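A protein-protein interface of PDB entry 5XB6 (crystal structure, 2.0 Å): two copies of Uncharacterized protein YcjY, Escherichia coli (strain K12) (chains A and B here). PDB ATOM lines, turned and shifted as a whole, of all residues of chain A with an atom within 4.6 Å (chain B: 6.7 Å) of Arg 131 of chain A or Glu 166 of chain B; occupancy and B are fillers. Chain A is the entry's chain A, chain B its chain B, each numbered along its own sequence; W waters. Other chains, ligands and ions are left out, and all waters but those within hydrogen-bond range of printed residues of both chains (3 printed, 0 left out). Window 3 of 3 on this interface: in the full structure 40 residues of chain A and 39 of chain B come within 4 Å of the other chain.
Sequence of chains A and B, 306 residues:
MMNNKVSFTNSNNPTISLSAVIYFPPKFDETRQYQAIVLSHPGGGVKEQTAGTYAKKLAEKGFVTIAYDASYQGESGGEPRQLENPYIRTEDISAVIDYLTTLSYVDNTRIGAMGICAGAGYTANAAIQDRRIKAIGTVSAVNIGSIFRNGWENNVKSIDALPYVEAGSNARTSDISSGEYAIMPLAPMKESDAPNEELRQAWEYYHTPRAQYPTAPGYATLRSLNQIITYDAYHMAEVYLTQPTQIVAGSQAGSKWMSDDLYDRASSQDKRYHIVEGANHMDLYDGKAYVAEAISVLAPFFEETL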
ATOM      1  N   ALA A 127      10.298   3.315  -5.171  1.00  0.00           N
ATOM      2  CA  ALA A 127      11.582   3.739  -5.707  1.00  0.00           C
ATOM      3  C   ALA A 127      11.894   2.881  -6.922  1.00  0.00           C
ATOM      4  O   ALA A 127      12.560   3.320  -7.874  1.00  0.00           O
ATOM      5  CB  ALA A 127      12.653   3.591  -4.658  1.00  0.00           C
ATOM      6  N   ILE A 128      11.395   1.650  -6.887  1.00  0.00           N
ATOM      7  CA  ILE A 128      11.679   0.733  -7.968  1.00  0.00           C
ATOM      8  C   ILE A 128      10.988   1.201  -9.235  1.00  0.00           C
ATOM      9  O   ILE A 128      11.589   1.177 -10.309  1.00  0.00           O
ATOM     10  CB  ILE A 128      11.307  -0.717  -7.608  1.00  0.00           C
ATOM     11  CG1 ILE A 128      12.414  -1.327  -6.746  1.00  0.00           C
ATOM     12  CG2 ILE A 128      11.101  -1.548  -8.871  1.00  0.00           C
ATOM     13  CD1 ILE A 128      12.055  -2.655  -6.083  1.00  0.00           C
ATOM     14  N   GLN A 129       9.756   1.689  -9.117  1.00  0.00           N
ATOM     15  CA  GLN A 129       8.996   1.982 -10.333  1.00  0.00           C
ATOM     16  C   GLN A 129       8.939   3.463 -10.664  1.00  0.00           C
ATOM     17  O   GLN A 129       8.663   3.830 -11.803  1.00  0.00           O
ATOM     18  CB  GLN A 129       7.586   1.379 -10.261  1.00  0.00           C
ATOM     19  CG  GLN A 129       6.707   1.945  -9.148  1.00  0.00           C
ATOM     20  CD  GLN A 129       5.336   1.287  -9.110  1.00  0.00           C
ATOM     21  OE1 GLN A 129       5.179   0.141  -9.526  1.00  0.00           O
ATOM     22  NE2 GLN A 129       4.335   2.019  -8.621  1.00  0.00           N
ATOM     23  N   ASP A 130       9.212   4.323  -9.686  1.00  0.00           N
ATOM     24  CA  ASP A 130       9.127   5.746  -9.939  1.00  0.00           C
ATOM     25  C   ASP A 130      10.513   6.353  -9.855  1.00  0.00           C
ATOM     26  O   ASP A 130      11.027   6.599  -8.755  1.00  0.00           O
ATOM     27  CB  ASP A 130       8.195   6.431  -8.934  1.00  0.00           C
ATOM     28  CG  ASP A 130       7.822   7.835  -9.354  1.00  0.00           C
ATOM     29  OD1 ASP A 130       8.636   8.506 -10.035  1.00  0.00           O
ATOM     30  OD2 ASP A 130       6.709   8.280  -9.013  1.00  0.00           O
ATOM     31  N   ARG A 131      11.106   6.609 -11.020  1.00  0.00           N
ATOM     32  CA  ARG A 131      12.499   7.051 -11.109  1.00  0.00           C
ATOM     33  C   ARG A 131      12.695   8.497 -10.691  1.00  0.00           C
ATOM     34  O   ARG A 131      13.825   8.992 -10.662  1.00  0.00           O
ATOM     35  CB  ARG A 131      13.031   6.841 -12.531  1.00  0.00           C
ATOM     36  CG  ARG A 131      12.871   5.406 -13.052  1.00  0.00           C
ATOM     37  CD  ARG A 131      13.250   4.360 -12.005  1.00  0.00           C
ATOM     38  NE  ARG A 131      14.667   4.405 -11.628  1.00  0.00           N
ATOM     39  CZ  ARG A 131      15.270   3.498 -10.860  1.00  0.00           C
ATOM     40  NH1 ARG A 131      14.581   2.469 -10.378  1.00  0.00           N
ATOM     41  NH2 ARG A 131      16.562   3.611 -10.579  1.00  0.00           N
ATOM     42  N   ARG A 132      11.605   9.184 -10.368  1.00  0.00           N
ATOM     43  CA  ARG A 132      11.705  10.541  -9.840  1.00  0.00           C
ATOM     44  C   ARG A 132      12.159  10.537  -8.383  1.00  0.00           C
ATOM     45  O   ARG A 132      12.540  11.577  -7.828  1.00  0.00           O
ATOM     46  CB  ARG A 132      10.371  11.282  -9.999  1.00  0.00           C
ATOM     47  CG  ARG A 132       9.936  11.454 -11.457  1.00  0.00           C
ATOM     48  CD  ARG A 132       8.525  12.000 -11.570  1.00  0.00           C
ATOM     49  NE  ARG A 132       7.574  11.126 -10.893  1.00  0.00           N
ATOM     50  CZ  ARG A 132       6.280  11.390 -10.753  1.00  0.00           C
ATOM     51  NH1 ARG A 132       5.784  12.513 -11.248  1.00  0.00           N
ATOM     52  NH2 ARG A 132       5.486  10.535 -10.099  1.00  0.00           N
ATOM     53  N   ILE A 133      12.110   9.367  -7.759  1.00  0.00           N
ATOM     54  CA  ILE A 133      12.578   9.209  -6.382  1.00  0.00           C
ATOM     55  C   ILE A 133      14.086   9.059  -6.423  1.00  0.00           C
ATOM     56  O   ILE A 133      14.605   8.112  -7.020  1.00  0.00           O
ATOM     57  CB  ILE A 133      11.959   7.969  -5.718  1.00  0.00           C
ATOM     58  CG1 ILE A 133      10.492   8.232  -5.396  1.00  0.00           C
ATOM     59  CG2 ILE A 133      12.715   7.606  -4.451  1.00  0.00           C
ATOM     60  CD1 ILE A 133       9.716   6.981  -5.025  1.00  0.00           C
ATOM     61  N   TYR A 240      16.397  -2.824 -10.264  1.00  0.00           N
ATOM     62  CA  TYR A 240      15.969  -1.429 -10.392  1.00  0.00           C
ATOM     63  C   TYR A 240      16.175  -0.567  -9.152  1.00  0.00           C
ATOM     64  O   TYR A 240      16.265   0.660  -9.261  1.00  0.00           O
ATOM     65  CB  TYR A 240      14.510  -1.346 -10.871  1.00  0.00           C
ATOM     66  CG  TYR A 240      14.296  -1.947 -12.237  1.00  0.00           C
ATOM     67  CD1 TYR A 240      14.934  -1.414 -13.356  1.00  0.00           C
ATOM     68  CD2 TYR A 240      13.461  -3.043 -12.419  1.00  0.00           C
ATOM     69  CE1 TYR A 240      14.749  -1.958 -14.616  1.00  0.00           C
ATOM     70  CE2 TYR A 240      13.268  -3.596 -13.679  1.00  0.00           C
ATOM     71  CZ  TYR A 240      13.917  -3.047 -14.772  1.00  0.00           C
ATOM     72  OH  TYR A 240      13.732  -3.594 -16.032  1.00  0.00           O
ATOM     73  N   THR A 242      18.238   1.146  -7.402  1.00  0.00           N
ATOM     74  CA  THR A 242      19.600   1.634  -7.548  1.00  0.00           C
ATOM     75  C   THR A 242      19.828   2.905  -6.739  1.00  0.00           C
ATOM     76  O   THR A 242      20.971   3.263  -6.458  1.00  0.00           O
ATOM     77  CB  THR A 242      19.916   1.934  -9.020  1.00  0.00           C
ATOM     78  OG1 THR A 242      18.978   2.894  -9.521  1.00  0.00           O
ATOM     79  CG2 THR A 242      19.845   0.681  -9.858  1.00  0.00           C
ATOM     80  N   GLN A 243      18.748   3.601  -6.393  1.00  0.00           N
ATOM     81  CA  GLN A 243      18.872   4.882  -5.706  1.00  0.00           C
ATOM     82  C   GLN A 243      19.541   4.677  -4.350  1.00  0.00           C
ATOM     83  O   GLN A 243      19.482   3.585  -3.786  1.00  0.00           O
ATOM     84  CB  GLN A 243      17.505   5.562  -5.520  1.00  0.00           C
ATOM     85  CG  GLN A 243      16.742   5.861  -6.810  1.00  0.00           C
ATOM     86  CD  GLN A 243      15.802   4.731  -7.219  1.00  0.00           C
ATOM     87  OE1 GLN A 243      16.152   3.555  -7.134  1.00  0.00           O
ATOM     88  NE2 GLN A 243      14.592   5.092  -7.660  1.00  0.00           N
ATOM     89  N   ALA B 161      16.165  -1.710 -19.792  1.00  0.00           N
ATOM     90  CA  ALA B 161      14.825  -1.158 -19.946  1.00  0.00           C
ATOM     91  C   ALA B 161      14.590   0.022 -18.999  1.00  0.00           C
ATOM     92  O   ALA B 161      13.507   0.599 -18.993  1.00  0.00           O
ATOM     93  CB  ALA B 161      13.774  -2.241 -19.726  1.00  0.00           C
ATOM     94  N   LEU B 162      15.596   0.386 -18.203  1.00  0.00           N
ATOM     95  CA  LEU B 162      15.461   1.542 -17.301  1.00  0.00           C
ATOM     96  C   LEU B 162      14.937   2.859 -17.935  1.00  0.00           C
ATOM     97  O   LEU B 162      14.133   3.553 -17.310  1.00  0.00           O
ATOM     98  CB  LEU B 162      16.765   1.795 -16.527  1.00  0.00           C
ATOM     99  CG  LEU B 162      16.722   2.793 -15.368  1.00  0.00           C
ATOM    100  CD1 LEU B 162      15.720   2.357 -14.288  1.00  0.00           C
ATOM    101  CD2 LEU B 162      18.110   3.005 -14.763  1.00  0.00           C
ATOM    102  N   PRO B 163      15.385   3.219 -19.159  1.00  0.00           N
ATOM    103  CA  PRO B 163      14.846   4.466 -19.732  1.00  0.00           C
ATOM    104  C   PRO B 163      13.329   4.426 -19.952  1.00  0.00           C
ATOM    105  O   PRO B 163      12.680   5.474 -20.004  1.00  0.00           O
ATOM    106  CB  PRO B 163      15.570   4.576 -21.082  1.00  0.00           C
ATOM    107  CG  PRO B 163      16.846   3.838 -20.879  1.00  0.00           C
ATOM    108  CD  PRO B 163      16.507   2.692 -19.958  1.00  0.00           C
ATOM    109  N   TYR B 164      12.777   3.222 -20.077  1.00  0.00           N
ATOM    110  CA  TYR B 164      11.328   3.051 -20.190  1.00  0.00           C
ATOM    111  C   TYR B 164      10.643   3.274 -18.845  1.00  0.00           C
ATOM    112  O   TYR B 164       9.544   3.835 -18.778  1.00  0.00           O
ATOM    113  CB  TYR B 164      11.001   1.656 -20.707  1.00  0.00           C
ATOM    114  CG  TYR B 164      11.491   1.412 -22.113  1.00  0.00           C
ATOM    115  CD1 TYR B 164      11.170   2.290 -23.147  1.00  0.00           C
ATOM    116  CD2 TYR B 164      12.280   0.306 -22.409  1.00  0.00           C
ATOM    117  CE1 TYR B 164      11.619   2.061 -24.442  1.00  0.00           C
ATOM    118  CE2 TYR B 164      12.731   0.073 -23.695  1.00  0.00           C
ATOM    119  CZ  TYR B 164      12.399   0.954 -24.706  1.00  0.00           C
ATOM    120  OH  TYR B 164      12.850   0.728 -25.987  1.00  0.00           O
ATOM    121  N   VAL B 165      11.282   2.820 -17.772  1.00  0.00           N
ATOM    122  CA  VAL B 165      10.751   3.094 -16.445  1.00  0.00           C
ATOM    123  C   VAL B 165      10.790   4.603 -16.234  1.00  0.00           C
ATOM    124  O   VAL B 165       9.809   5.212 -15.774  1.00  0.00           O
ATOM    125  CB  VAL B 165      11.535   2.364 -15.352  1.00  0.00           C
ATOM    126  CG1 VAL B 165      10.761   2.417 -14.022  1.00  0.00           C
ATOM    127  CG2 VAL B 165      11.797   0.913 -15.759  1.00  0.00           C
ATOM    128  N   GLU B 166      11.915   5.216 -16.602  1.00  0.00           N
ATOM    129  CA  GLU B 166      12.042   6.671 -16.519  1.00  0.00           C
ATOM    130  C   GLU B 166      10.951   7.365 -17.327  1.00  0.00           C
ATOM    131  O   GLU B 166      10.339   8.330 -16.857  1.00  0.00           O
ATOM    132  CB  GLU B 166      13.441   7.127 -16.962  1.00  0.00           C
ATOM    133  CG  GLU B 166      14.556   6.675 -16.012  1.00  0.00           C
ATOM    134  CD  GLU B 166      15.959   7.036 -16.489  1.00  0.00           C
ATOM    135  OE1 GLU B 166      16.086   7.836 -17.441  1.00  0.00           O
ATOM    136  OE2 GLU B 166      16.937   6.515 -15.904  1.00  0.00           O
ATOM    137  N   ALA B 167      10.699   6.862 -18.533  1.00  0.00           N
ATOM    138  CA  ALA B 167       9.690   7.457 -19.405  1.00  0.00           C
ATOM    139  C   ALA B 167       8.292   7.397 -18.789  1.00  0.00           C
ATOM    140  O   ALA B 167       7.510   8.337 -18.914  1.00  0.00           O
ATOM    141  CB  ALA B 167       9.714   6.797 -20.786  1.00  0.00           C
ATOM    142  N   GLY B 168       7.970   6.293 -18.116  1.00  0.00           N
ATOM    143  CA  GLY B 168       6.668   6.195 -17.469  1.00  0.00           C
ATOM    144  C   GLY B 168       6.582   7.132 -16.273  1.00  0.00           C
ATOM    145  O   GLY B 168       5.518   7.688 -15.952  1.00  0.00           O
ATOM    146  N   SER B 169       7.709   7.303 -15.593  1.00  0.00           N
ATOM    147  CA  SER B 169       7.751   8.192 -14.443  1.00  0.00           C
ATOM    148  C   SER B 169       7.569   9.640 -14.877  1.00  0.00           C
ATOM    149  O   SER B 169       6.795  10.389 -14.268  1.00  0.00           O
ATOM    150  CB  SER B 169       9.062   8.020 -13.687  1.00  0.00           C
ATOM    151  OG  SER B 169       9.208   6.686 -13.264  1.00  0.00           O
ATOM    152  N   ASN B 170       8.265  10.039 -15.938  1.00  0.00           N
ATOM    153  CA  ASN B 170       8.193  11.432 -16.367  1.00  0.00           C
ATOM    154  C   ASN B 170       6.844  11.759 -16.991  1.00  0.00           C
ATOM    155  O   ASN B 170       6.405  12.911 -16.983  1.00  0.00           O
ATOM    156  CB  ASN B 170       9.351  11.780 -17.304  1.00  0.00           C
ATOM    157  CG  ASN B 170      10.696  11.707 -16.611  1.00  0.00           C
ATOM    158  OD1 ASN B 170      10.812  12.015 -15.424  1.00  0.00           O
ATOM    159  ND2 ASN B 170      11.719  11.284 -17.346  1.00  0.00           N
ATOM    160  N   ALA B 171       6.176  10.732 -17.510  1.00  0.00           N
ATOM    161  CA  ALA B 171       4.841  10.894 -18.078  1.00  0.00           C
ATOM    162  C   ALA B 171       3.881  11.384 -17.002  1.00  0.00           C
ATOM    163  O   ALA B 171       2.987  12.195 -17.254  1.00  0.00           O
ATOM    164  CB  ALA B 171       4.353   9.565 -18.671  1.00  0.00           C
ATOM    165  N   ASN B 226       5.927   2.554 -16.499  1.00  0.00           N
ATOM    166  CA  ASN B 226       6.783   2.229 -15.358  1.00  0.00           C
ATOM    167  C   ASN B 226       6.260   1.046 -14.527  1.00  0.00           C
ATOM    168  O   ASN B 226       7.054   0.207 -14.059  1.00  0.00           O
ATOM    169  CB  ASN B 226       7.103   3.467 -14.503  1.00  0.00           C
ATOM    170  CG  ASN B 226       5.892   4.013 -13.757  1.00  0.00           C
ATOM    171  OD1 ASN B 226       4.748   3.844 -14.184  1.00  0.00           O
ATOM    172  ND2 ASN B 226       6.148   4.697 -12.641  1.00  0.00           N
ATOM    173  N   THR B 230       8.137  -3.068 -14.485  1.00  0.00           N
ATOM    174  CA  THR B 230       8.473  -3.688 -13.207  1.00  0.00           C
ATOM    175  C   THR B 230       7.458  -4.760 -12.787  1.00  0.00           C
ATOM    176  O   THR B 230       7.378  -5.124 -11.616  1.00  0.00           O
ATOM    177  CB  THR B 230       8.614  -2.624 -12.106  1.00  0.00           C
ATOM    178  OG1 THR B 230       7.442  -1.797 -12.084  1.00  0.00           O
ATOM    179  CG2 THR B 230       9.830  -1.741 -12.388  1.00  0.00           C
HETATM  180  O   HOH W   1       4.147   4.826 -10.320  1.00  0.00           O
HETATM  181  O   HOH W   2       5.102  -2.479 -11.055  1.00  0.00           O
HETATM  182  O   HOH W   3      16.465   6.221 -12.948  1.00  0.00           O
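No position is printed for both chains.
Of the 14 pairs that touch across the chains among the printed residues, none has its exchanged pair printed and touching as well.
O of Gln 129 of chain A is in hydrogen-bond range of OG of Ser 169 of chain B.
The backbone carbonyl oxygen (O) of Gln 129 of chain A sits at hydrogen-bond distance from the side-chain amide nitrogen (ND2) of Asn 226 of chain B (2.8 Å).
The backbone NH of Arg 131 of chain A sits at hydrogen-bond distance from the side-chain hydroxyl of Ser 169 of chain B (2.9 Å).
CG2 of Thr 230 of chain B touches CG2 of Ile 128 of chain A, 3.7 Å away.
Gln 129 of chain A touches Val 165 of chain B (O to CG1, 3.4 Å).
Gln 129 of chain A touches Thr 230 of chain B (CB to OG1, 3.7 Å).
Asp 130 of chain A touches Ser 169 of chain B (CA to OG, 3.5 Å).
CD1 of Leu 162 of chain B touches NE of Arg 131 of chain A (3.5 Å).
Val 165 of chain B touches Arg 131 of chain A.
Arg 131 of chain A touches Glu 166 of chain B (CG to CG, 3.6 Å).
NE of Arg 132 of chain A touches O of Ser 169 of chain B, at 3.5 Å.
Ala 161 of chain B touches Tyr 240 of chain A (CB to OH, 3.9 Å).
CG2 of Thr 230 of chain B touches CD2 of Tyr 240 of chain A, at 3.9 Å.
O of Ala 127 of chain A lies within hydrogen-bond range of NH1 of Arg 131 of chain A, 3.3 Å away.
The backbone carbonyl oxygen (O) of Ile 128 of chain A sits at hydrogen-bond distance from the guanidinium group (NH1) of Arg 131 of chain A, at 3.3 Å.
The side-chain carboxylate of Asp 130 of chain A lies within salt-bridge range of the guanidinium group of Arg 132 of chain A (2.8 Å).
The side-chain hydroxyl (OG1) of Thr 242 of chain A lies within hydrogen-bond range of the guanidinium group (NH2) of Arg 131 of chain A (2.7 Å).
The guanidinium group of Arg 131 of chain A sits at hydrogen-bond distance from the side-chain amide oxygen of Gln 243 of chain A, at 3.5 Å.
OG of Ser 169 of chain B is in hydrogen-bond range of O of Val 165 of chain B, at 3.0 Å.
Of the printed residues of chain B, Ile 128 of chain A touches Thr 230.
Of chain B, only Leu 162 (3.5 Å), Val 165 (3.7 Å), Glu 166 (3.6 Å) and Ser 169 (2.9 Å) come within 4 Å of Arg 131 of chain A.
Printed residues of chain B within 4 Å of Tyr 240 of chain A: Ala 161 (3.9 Å), Leu 162 (3.96 Å) and Thr 230 (3.9 Å).
Gln 243 of chain A touches none of the printed residues of chain B.
Of the printed residues of chain A, Leu 162 of chain B touches Arg 131 (3.5 Å) and Tyr 240 (3.96 Å).
Of the printed residues of chain A, Val 165 of chain B touches Gln 129 (3.4 Å) and Arg 131 (3.7 Å).
Of chain A, only Arg 131 comes within 4 Å of Glu 166 of chain B.
Ala 171 of chain B touches none of the printed residues of chain A.
Printed residues of chain A within 4 Å of Thr 230 of chain B: Ile 128 (3.7 Å), Gln 129 (3.7 Å) and Tyr 240 (3.9 Å).
The nearest printed residue of chain A that does not touch Glu 166 of chain B is Gln 129 of chain A (6.0 Å).
The nearest printed residue of chain A that does not touch Ala 161 of chain B is Arg 131 of chain A (7.7 Å).
Water W2 lies within hydrogen-bond range of OG1 of Thr 230 of chain B (2.6 Å) and OE1 of Gln 129 of chain A (3.0 Å).
Water W3 lies within hydrogen-bond range of the guanidinium group (NE) of Arg 131 of chain A (2.9 Å) and the side-chain carboxylate (OE2) of Glu 166 of chain B (3.0 Å).
Water W1 lies within hydrogen-bond range of the side-chain amide nitrogen (ND2) of Asn 226 of chain B and the side-chain amide nitrogen (NE2) of Gln 129 of chain A.
Hydrophobic or aromatic side chains of chain A that line the printed part of chain B: Ile 128 and Tyr 240.
Hydrophobic or aromatic side chains of chain B within 4 Å of the printed part of chain A: Ala 161, Leu 162 and Val 165.
Among the printed residues, 14 pairs touch across the chains.
Among the printed residues, no Asp or Glu carboxylate lies within 4 Å of a Lys or Arg side-chain nitrogen of the other chain.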
